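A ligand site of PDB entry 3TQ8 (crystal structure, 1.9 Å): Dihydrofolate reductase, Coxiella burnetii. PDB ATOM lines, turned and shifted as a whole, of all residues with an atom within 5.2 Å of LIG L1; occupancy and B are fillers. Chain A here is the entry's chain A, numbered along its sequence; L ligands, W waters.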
ATOM      1  N   ILE A   6      17.705  12.659  16.100  1.00  0.00           N
ATOM      2  CA  ILE A   6      16.535  12.187  15.351  1.00  0.00           C
ATOM      3  C   ILE A   6      15.991  11.012  16.142  1.00  0.00           C
ATOM      4  O   ILE A   6      16.754  10.147  16.582  1.00  0.00           O
ATOM      5  CB  ILE A   6      16.876  11.834  13.870  1.00  0.00           C
ATOM      6  CG1 ILE A   6      15.598  11.499  13.088  1.00  0.00           C
ATOM      7  CG2 ILE A   6      17.925  10.675  13.792  1.00  0.00           C
ATOM      8  CD1 ILE A   6      15.770  11.512  11.578  1.00  0.00           C
ATOM      9  N   ALA A   7      14.683  11.005  16.392  1.00  0.00           N
ATOM     10  CA  ALA A   7      14.070   9.950  17.172  1.00  0.00           C
ATOM     11  C   ALA A   7      12.610   9.830  16.793  1.00  0.00           C
ATOM     12  O   ALA A   7      11.983  10.814  16.352  1.00  0.00           O
ATOM     13  CB  ALA A   7      14.214  10.244  18.667  1.00  0.00           C
ATOM     14  N   ALA A   8      12.083   8.622  16.981  1.00  0.00           N
ATOM     15  CA  ALA A   8      10.668   8.345  16.870  1.00  0.00           C
ATOM     16  C   ALA A   8      10.153   7.957  18.235  1.00  0.00           C
ATOM     17  O   ALA A   8      10.696   7.066  18.886  1.00  0.00           O
ATOM     18  CB  ALA A   8      10.376   7.213  15.868  1.00  0.00           C
ATOM     19  N   GLU A  20      14.075  -3.242  21.180  1.00  0.00           N
ATOM     20  CA  GLU A  20      13.434  -3.174  19.880  1.00  0.00           C
ATOM     21  C   GLU A  20      12.534  -1.936  19.853  1.00  0.00           C
ATOM     22  O   GLU A  20      12.190  -1.380  20.898  1.00  0.00           O
ATOM     23  CB  GLU A  20      12.562  -4.397  19.624  1.00  0.00           C
ATOM     24  CG  GLU A  20      13.256  -5.728  19.825  1.00  0.00           C
ATOM     25  CD  GLU A  20      12.402  -6.894  19.303  1.00  0.00           C
ATOM     26  OE1 GLU A  20      11.266  -7.086  19.802  1.00  0.00           O
ATOM     27  OE2 GLU A  20      12.865  -7.611  18.401  1.00  0.00           O
ATOM     28  N   LEU A  21      12.143  -1.528  18.655  1.00  0.00           N
ATOM     29  CA  LEU A  21      11.109  -0.518  18.474  1.00  0.00           C
ATOM     30  C   LEU A  21       9.770  -1.092  18.917  1.00  0.00           C
ATOM     31  O   LEU A  21       9.524  -2.299  18.737  1.00  0.00           O
ATOM     32  CB  LEU A  21      11.027  -0.075  17.002  1.00  0.00           C
ATOM     33  CG  LEU A  21      12.279   0.613  16.447  1.00  0.00           C
ATOM     34  CD1 LEU A  21      12.067   0.988  14.978  1.00  0.00           C
ATOM     35  CD2 LEU A  21      12.661   1.853  17.260  1.00  0.00           C
ATOM     36  N   ASP A  28       7.925   6.500   9.076  1.00  0.00           N
ATOM     37  CA  ASP A  28       9.078   6.903   9.863  1.00  0.00           C
ATOM     38  C   ASP A  28      10.391   6.342   9.323  1.00  0.00           C
ATOM     39  O   ASP A  28      11.381   7.049   9.276  1.00  0.00           O
ATOM     40  CB  ASP A  28       8.976   6.492  11.323  1.00  0.00           C
ATOM     41  CG  ASP A  28      10.226   6.850  12.077  1.00  0.00           C
ATOM     42  OD1 ASP A  28      10.431   8.064  12.255  1.00  0.00           O
ATOM     43  OD2 ASP A  28      11.023   5.944  12.418  1.00  0.00           O
ATOM     44  N   LEU A  29      10.395   5.069   8.917  1.00  0.00           N
ATOM     45  CA  LEU A  29      11.623   4.467   8.398  1.00  0.00           C
ATOM     46  C   LEU A  29      12.085   5.167   7.105  1.00  0.00           C
ATOM     47  O   LEU A  29      13.291   5.356   6.904  1.00  0.00           O
ATOM     48  CB  LEU A  29      11.454   2.962   8.190  1.00  0.00           C
ATOM     49  CG  LEU A  29      11.184   2.142   9.462  1.00  0.00           C
ATOM     50  CD1 LEU A  29      10.979   0.657   9.131  1.00  0.00           C
ATOM     51  CD2 LEU A  29      12.299   2.316  10.493  1.00  0.00           C
ATOM     52  N   HIS A  31      11.394   8.357   6.223  1.00  0.00           N
ATOM     53  CA  HIS A  31      11.806   9.669   6.744  1.00  0.00           C
ATOM     54  C   HIS A  31      13.222   9.622   7.330  1.00  0.00           C
ATOM     55  O   HIS A  31      14.063  10.447   6.980  1.00  0.00           O
ATOM     56  CB  HIS A  31      10.754  10.117   7.802  1.00  0.00           C
ATOM     57  CG  HIS A  31      11.215  11.159   8.784  1.00  0.00           C
ATOM     58  ND1 HIS A  31      11.149  12.517   8.516  1.00  0.00           N
ATOM     59  CD2 HIS A  31      11.654  11.050  10.049  1.00  0.00           C
ATOM     60  CE1 HIS A  31      11.561  13.189   9.575  1.00  0.00           C
ATOM     61  NE2 HIS A  31      11.882  12.318  10.519  1.00  0.00           N
ATOM     62  N   PHE A  32      13.485   8.649   8.200  1.00  0.00           N
ATOM     63  CA  PHE A  32      14.787   8.489   8.837  1.00  0.00           C
ATOM     64  C   PHE A  32      15.901   8.263   7.829  1.00  0.00           C
ATOM     65  O   PHE A  32      16.963   8.907   7.892  1.00  0.00           O
ATOM     66  CB  PHE A  32      14.726   7.323   9.826  1.00  0.00           C
ATOM     67  CG  PHE A  32      16.057   6.935  10.397  1.00  0.00           C
ATOM     68  CD1 PHE A  32      16.601   7.640  11.472  1.00  0.00           C
ATOM     69  CD2 PHE A  32      16.761   5.850   9.894  1.00  0.00           C
ATOM     70  CE1 PHE A  32      17.824   7.299  12.005  1.00  0.00           C
ATOM     71  CE2 PHE A  32      17.988   5.482  10.443  1.00  0.00           C
ATOM     72  CZ  PHE A  32      18.528   6.214  11.503  1.00  0.00           C
ATOM     73  N   THR A  47      21.798   0.018  20.577  1.00  0.00           N
ATOM     74  CA  THR A  47      21.088   0.350  19.349  1.00  0.00           C
ATOM     75  C   THR A  47      21.726  -0.329  18.134  1.00  0.00           C
ATOM     76  O   THR A  47      21.005  -0.881  17.289  1.00  0.00           O
ATOM     77  CB  THR A  47      20.973   1.872  19.158  1.00  0.00           C
ATOM     78  OG1 THR A  47      20.136   2.396  20.198  1.00  0.00           O
ATOM     79  CG2 THR A  47      20.346   2.214  17.829  1.00  0.00           C
ATOM     80  N   SER A  50      20.580  -3.852  18.343  1.00  0.00           N
ATOM     81  CA  SER A  50      19.193  -3.907  17.885  1.00  0.00           C
ATOM     82  C   SER A  50      19.084  -3.895  16.358  1.00  0.00           C
ATOM     83  O   SER A  50      18.363  -4.700  15.771  1.00  0.00           O
ATOM     84  CB  SER A  50      18.392  -2.740  18.472  1.00  0.00           C
ATOM     85  OG  SER A  50      17.039  -2.820  18.078  1.00  0.00           O
ATOM     86  N   ILE A  51      19.805  -2.995  15.709  1.00  0.00           N
ATOM     87  CA  ILE A  51      19.805  -2.912  14.245  1.00  0.00           C
ATOM     88  C   ILE A  51      20.523  -4.116  13.614  1.00  0.00           C
ATOM     89  O   ILE A  51      20.105  -4.652  12.571  1.00  0.00           O
ATOM     90  CB  ILE A  51      20.392  -1.560  13.735  1.00  0.00           C
ATOM     91  CG1 ILE A  51      19.558  -0.404  14.279  1.00  0.00           C
ATOM     92  CG2 ILE A  51      20.390  -1.508  12.192  1.00  0.00           C
ATOM     93  CD1 ILE A  51      20.162   0.998  14.090  1.00  0.00           C
ATOM     94  N   LEU A  55      23.997   0.556   8.972  1.00  0.00           N
ATOM     95  CA  LEU A  55      23.028   1.123   8.028  1.00  0.00           C
ATOM     96  C   LEU A  55      23.769   1.502   6.756  1.00  0.00           C
ATOM     97  O   LEU A  55      24.750   2.223   6.815  1.00  0.00           O
ATOM     98  CB  LEU A  55      22.320   2.324   8.658  1.00  0.00           C
ATOM     99  CG  LEU A  55      21.537   2.035   9.939  1.00  0.00           C
ATOM    100  CD1 LEU A  55      21.049   3.326  10.553  1.00  0.00           C
ATOM    101  CD2 LEU A  55      20.335   1.101   9.688  1.00  0.00           C
ATOM    102  N   ILE A  95      22.683  12.131  15.819  1.00  0.00           N
ATOM    103  CA  ILE A  95      22.628  11.179  16.918  1.00  0.00           C
ATOM    104  C   ILE A  95      21.315  10.379  16.750  1.00  0.00           C
ATOM    105  O   ILE A  95      20.226  10.958  16.736  1.00  0.00           O
ATOM    106  CB  ILE A  95      22.634  11.882  18.297  1.00  0.00           C
ATOM    107  CG1 ILE A  95      23.761  12.942  18.422  1.00  0.00           C
ATOM    108  CG2 ILE A  95      22.738  10.851  19.423  1.00  0.00           C
ATOM    109  CD1 ILE A  95      25.133  12.450  18.226  1.00  0.00           C
ATOM    110  N   ILE A  96      21.426   9.060  16.630  1.00  0.00           N
ATOM    111  CA  ILE A  96      20.262   8.240  16.305  1.00  0.00           C
ATOM    112  C   ILE A  96      19.763   7.344  17.451  1.00  0.00           C
ATOM    113  O   ILE A  96      18.841   6.552  17.241  1.00  0.00           O
ATOM    114  CB  ILE A  96      20.479   7.353  15.033  1.00  0.00           C
ATOM    115  CG1 ILE A  96      21.490   6.227  15.308  1.00  0.00           C
ATOM    116  CG2 ILE A  96      20.863   8.227  13.821  1.00  0.00           C
ATOM    117  CD1 ILE A  96      21.413   5.099  14.308  1.00  0.00           C
ATOM    118  N   GLY A  97      20.346   7.480  18.632  1.00  0.00           N
ATOM    119  CA  GLY A  97      19.880   6.774  19.844  1.00  0.00           C
ATOM    120  C   GLY A  97      20.932   5.866  20.438  1.00  0.00           C
ATOM    121  O   GLY A  97      22.058   5.860  19.955  1.00  0.00           O
ATOM    122  N   PHE A 102      20.767   9.530  23.779  1.00  0.00           N
ATOM    123  CA  PHE A 102      19.910  10.714  23.670  1.00  0.00           C
ATOM    124  C   PHE A 102      19.998  11.591  24.934  1.00  0.00           C
ATOM    125  O   PHE A 102      20.146  12.800  24.840  1.00  0.00           O
ATOM    126  CB  PHE A 102      18.456  10.365  23.409  1.00  0.00           C
ATOM    127  CG  PHE A 102      18.146   9.888  21.991  1.00  0.00           C
ATOM    128  CD1 PHE A 102      18.681  10.498  20.875  1.00  0.00           C
ATOM    129  CD2 PHE A 102      17.242   8.857  21.801  1.00  0.00           C
ATOM    130  CE1 PHE A 102      18.343  10.061  19.592  1.00  0.00           C
ATOM    131  CE2 PHE A 102      16.904   8.420  20.517  1.00  0.00           C
ATOM    132  CZ  PHE A 102      17.472   9.022  19.418  1.00  0.00           C
ATOM    133  N   ILE A 113      14.863  16.306  15.297  1.00  0.00           N
ATOM    134  CA  ILE A 113      13.889  15.878  14.285  1.00  0.00           C
ATOM    135  C   ILE A 113      13.089  14.713  14.869  1.00  0.00           C
ATOM    136  O   ILE A 113      13.579  13.574  14.927  1.00  0.00           O
ATOM    137  CB  ILE A 113      14.578  15.468  12.956  1.00  0.00           C
ATOM    138  CG1 ILE A 113      15.466  16.614  12.425  1.00  0.00           C
ATOM    139  CG2 ILE A 113      13.533  15.074  11.899  1.00  0.00           C
ATOM    140  CD1 ILE A 113      16.267  16.310  11.174  1.00  0.00           C
ATOM    141  N   THR A 115       9.738  12.207  15.298  1.00  0.00           N
ATOM    142  CA  THR A 115       8.472  11.611  14.871  1.00  0.00           C
ATOM    143  C   THR A 115       7.683  11.342  16.142  1.00  0.00           C
ATOM    144  O   THR A 115       8.176  10.652  17.045  1.00  0.00           O
ATOM    145  CB  THR A 115       8.683  10.295  14.118  1.00  0.00           C
ATOM    146  OG1 THR A 115       9.553  10.536  13.007  1.00  0.00           O
ATOM    147  CG2 THR A 115       7.340   9.738  13.598  1.00  0.00           C
HETATM  148  C1  LIG L   1      14.544   5.509  13.605  1.00  0.00           C
HETATM  149  N1  LIG L   1      13.651   6.494  13.363  1.00  0.00           N
HETATM  150  C2  LIG L   1      13.836   7.763  13.823  1.00  0.00           C
HETATM  151  N2  LIG L   1      12.917   8.729  13.528  1.00  0.00           N
HETATM  152  N3  LIG L   1      14.924   8.093  14.557  1.00  0.00           N
HETATM  153  C3  LIG L   1      15.860   7.172  14.868  1.00  0.00           C
HETATM  154  N4  LIG L   1      16.903   7.555  15.610  1.00  0.00           N
HETATM  155  C4  LIG L   1      15.690   5.774  14.371  1.00  0.00           C
HETATM  156  C5  LIG L   1      16.761   4.741  14.688  1.00  0.00           C
HETATM  157  C6  LIG L   1      16.502   3.300  14.263  1.00  0.00           C
HETATM  158  C7  LIG L   1      16.447   2.908  12.920  1.00  0.00           C
HETATM  159  C8  LIG L   1      16.213   1.569  12.558  1.00  0.00           C
HETATM  160  O1  LIG L   1      16.161   1.138  11.249  1.00  0.00           O
HETATM  161  C9  LIG L   1      16.384   2.088  10.199  1.00  0.00           C
HETATM  162  C10 LIG L   1      16.024   0.561  13.607  1.00  0.00           C
HETATM  163  O2  LIG L   1      15.763  -0.755  13.303  1.00  0.00           O
HETATM  164  C11 LIG L   1      14.401  -1.018  12.965  1.00  0.00           C
HETATM  165  C12 LIG L   1      16.057   1.021  15.003  1.00  0.00           C
HETATM  166  O3  LIG L   1      15.881   0.109  15.999  1.00  0.00           O
HETATM  167  C13 LIG L   1      16.158   0.487  17.355  1.00  0.00           C
HETATM  168  C14 LIG L   1      16.302   2.371  15.279  1.00  0.00           C
HETATM  169  P1  LG2 L   2      22.027   2.835  23.830  1.00  0.00           P
HETATM  170  O1  LG2 L   2      21.992   4.266  24.186  1.00  0.00           O
HETATM  171  O2  LG2 L   2      21.643   2.544  22.423  1.00  0.00           O
HETATM  172  O3  LG2 L   2      23.440   2.132  24.122  1.00  0.00           O
HETATM  173  C1  LG2 L   2      23.898   2.079  25.456  1.00  0.00           C
HETATM  174  C2  LG2 L   2      25.329   1.603  25.388  1.00  0.00           C
HETATM  175  O4  LG2 L   2      26.076   2.535  24.635  1.00  0.00           O
HETATM  176  C3  LG2 L   2      26.005   1.461  26.733  1.00  0.00           C
HETATM  177  O5  LG2 L   2      25.651   0.223  27.320  1.00  0.00           O
HETATM  178  C4  LG2 L   2      27.455   1.621  26.322  1.00  0.00           C
HETATM  179  O6  LG2 L   2      27.952   0.497  25.613  1.00  0.00           O
HETATM  180  C5  LG2 L   2      27.350   2.688  25.248  1.00  0.00           C
HETATM  181  N1  LG2 L   2      27.478   4.082  25.689  1.00  0.00           N
HETATM  182  C6  LG2 L   2      26.488   5.038  25.762  1.00  0.00           C
HETATM  183  N2  LG2 L   2      27.046   6.202  26.172  1.00  0.00           N
HETATM  184  C7  LG2 L   2      28.374   6.003  26.341  1.00  0.00           C
HETATM  185  C8  LG2 L   2      29.401   6.851  26.749  1.00  0.00           C
HETATM  186  N3  LG2 L   2      29.161   8.117  27.038  1.00  0.00           N
HETATM  187  N4  LG2 L   2      30.686   6.348  26.828  1.00  0.00           N
HETATM  188  C9  LG2 L   2      30.937   5.038  26.500  1.00  0.00           C
HETATM  189  N5  LG2 L   2      29.916   4.201  26.108  1.00  0.00           N
HETATM  190  C10 LG2 L   2      28.656   4.679  26.037  1.00  0.00           C
HETATM  191  O7  LG2 L   2      21.159   1.935  24.819  1.00  0.00           O
HETATM  192  P2  LG2 L   2      19.691   2.136  25.419  1.00  0.00           P
HETATM  193  O8  LG2 L   2      19.628   3.336  26.265  1.00  0.00           O
HETATM  194  O9  LG2 L   2      19.427   0.811  26.014  1.00  0.00           O
HETATM  195  O10 LG2 L   2      18.747   2.346  24.121  1.00  0.00           O
HETATM  196  C11 LG2 L   2      18.268   1.282  23.332  1.00  0.00           C
HETATM  197  C12 LG2 L   2      16.735   1.355  23.220  1.00  0.00           C
HETATM  198  O11 LG2 L   2      16.361   2.525  22.505  1.00  0.00           O
HETATM  199  C13 LG2 L   2      16.159   0.186  22.447  1.00  0.00           C
HETATM  200  O12 LG2 L   2      14.935  -0.197  23.000  1.00  0.00           O
HETATM  201  C14 LG2 L   2      15.936   0.714  21.049  1.00  0.00           C
HETATM  202  O13 LG2 L   2      14.920   0.030  20.312  1.00  0.00           O
HETATM  203  C15 LG2 L   2      15.579   2.155  21.371  1.00  0.00           C
HETATM  204  N6  LG2 L   2      15.821   3.007  20.189  1.00  0.00           N
HETATM  205  C16 LG2 L   2      14.744   3.708  19.735  1.00  0.00           C
HETATM  206  C17 LG2 L   2      14.864   4.752  18.838  1.00  0.00           C
HETATM  207  C18 LG2 L   2      13.651   5.466  18.378  1.00  0.00           C
HETATM  208  O14 LG2 L   2      13.884   6.536  17.534  1.00  0.00           O
HETATM  209  N7  LG2 L   2      12.425   5.117  18.786  1.00  0.00           N
HETATM  210  C19 LG2 L   2      16.252   5.136  18.372  1.00  0.00           C
HETATM  211  C20 LG2 L   2      17.384   4.311  18.896  1.00  0.00           C
HETATM  212  C21 LG2 L   2      17.101   3.289  19.791  1.00  0.00           C
HETATM  213  P3  LG2 L   2      28.740  -0.764  26.241  1.00  0.00           P
HETATM  214  O15 LG2 L   2      27.702  -1.475  27.040  1.00  0.00           O
HETATM  215  O16 LG2 L   2      29.216  -1.652  25.119  1.00  0.00           O
HETATM  216  O17 LG2 L   2      29.897  -0.224  27.028  1.00  0.00           O
HETATM  217  O   HOH W   1      15.118   3.567   7.657  1.00  0.00           O
HETATM  218  O   HOH W   2      15.785  -2.611  15.682  1.00  0.00           O
HETATM  219  O   HOH W   3      12.229  11.714  13.342  1.00  0.00           O
HETATM  220  O   HOH W   4      17.029  -1.389  10.486  1.00  0.00           O
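A nitrogen (N4) of LIG L1 is in hydrogen-bond range of the backbone carbonyl oxygen of Ile 96 (2.7 Å). O of Ile 6 is in hydrogen-bond range of N4 of LIG L1, at 2.8 Å. A nitrogen (N1) of LIG L1 sits at hydrogen-bond distance from the side-chain carboxylate of Asp 28, 2.8 Å away. The backbone NH (N) of Ala 7 lies close to a nitrogen (N3) of LIG L1 (3.5 Å). The backbone NH of Ala 8 lies within hydrogen-bond range of an oxygen (O14) of LG2 L2 (2.8 Å). A nitrogen (N7) of LG2 L2 is in hydrogen-bond range of the backbone carbonyl oxygen of Ala 8 (2.6 Å). O2 of LG2 L2 sits at hydrogen-bond distance from N of Thr 47 (3.1 Å). OG1 of Thr 47 is in hydrogen-bond range of O2 of LG2 L2, at 2.7 Å. An oxygen (O13) of LG2 L2 sits close to the backbone NH (N) of Glu 20 (3.5 Å). O13 of LG2 L2 lies close to O of Glu 20, at 3.1 Å.
Water W2 bridges OG of Ser 50 (2.7 Å) and O3 of LIG L1 (2.7 Å). Water W3 lies within hydrogen-bond range of O of Ile 113 (2.8 Å), NE2 of His 31 (2.9 Å), OG1 of Thr 115 (2.9 Å), N2 of LIG L1 (3.1 Å) and O of Ala 7 (3.2 Å).
Residues that only touch LIG L1: Ala 8 (3.6 Å), Leu 21 (3.7 Å), Phe 32 (3.5 Å), Ser 50 (3.5 Å), Ile 51 (3.7 Å) and Thr 115 (3.9 Å). Hydrophobic or aromatic side chains within 4 Å of LIG L1: Ile 6, Ala 8, Leu 21, Phe 32, Ile 51 and Ile 96. Ten residues have an atom within 4 Å of LIG L1: Ile 6, Ala 7, Ala 8, Leu 21, Asp 28, Phe 32, Ser 50, Ile 51, Ile 96 and Thr 115.
The backbone NH (N) of Ile 6 lies within hydrogen-bond range of the backbone carbonyl oxygen (O) of Ile 95 (3.1 Å). The side-chain carboxylate of Asp 28 sits at hydrogen-bond distance from the side-chain hydroxyl of Thr 115, 2.7 Å away. The backbone NH (N) of Thr 115 sits at hydrogen-bond distance from the backbone carbonyl oxygen (O) of Ala 7 (2.8 Å). O of Ile 113 is in hydrogen-bond range of N of Ala 7 (3.2 Å).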
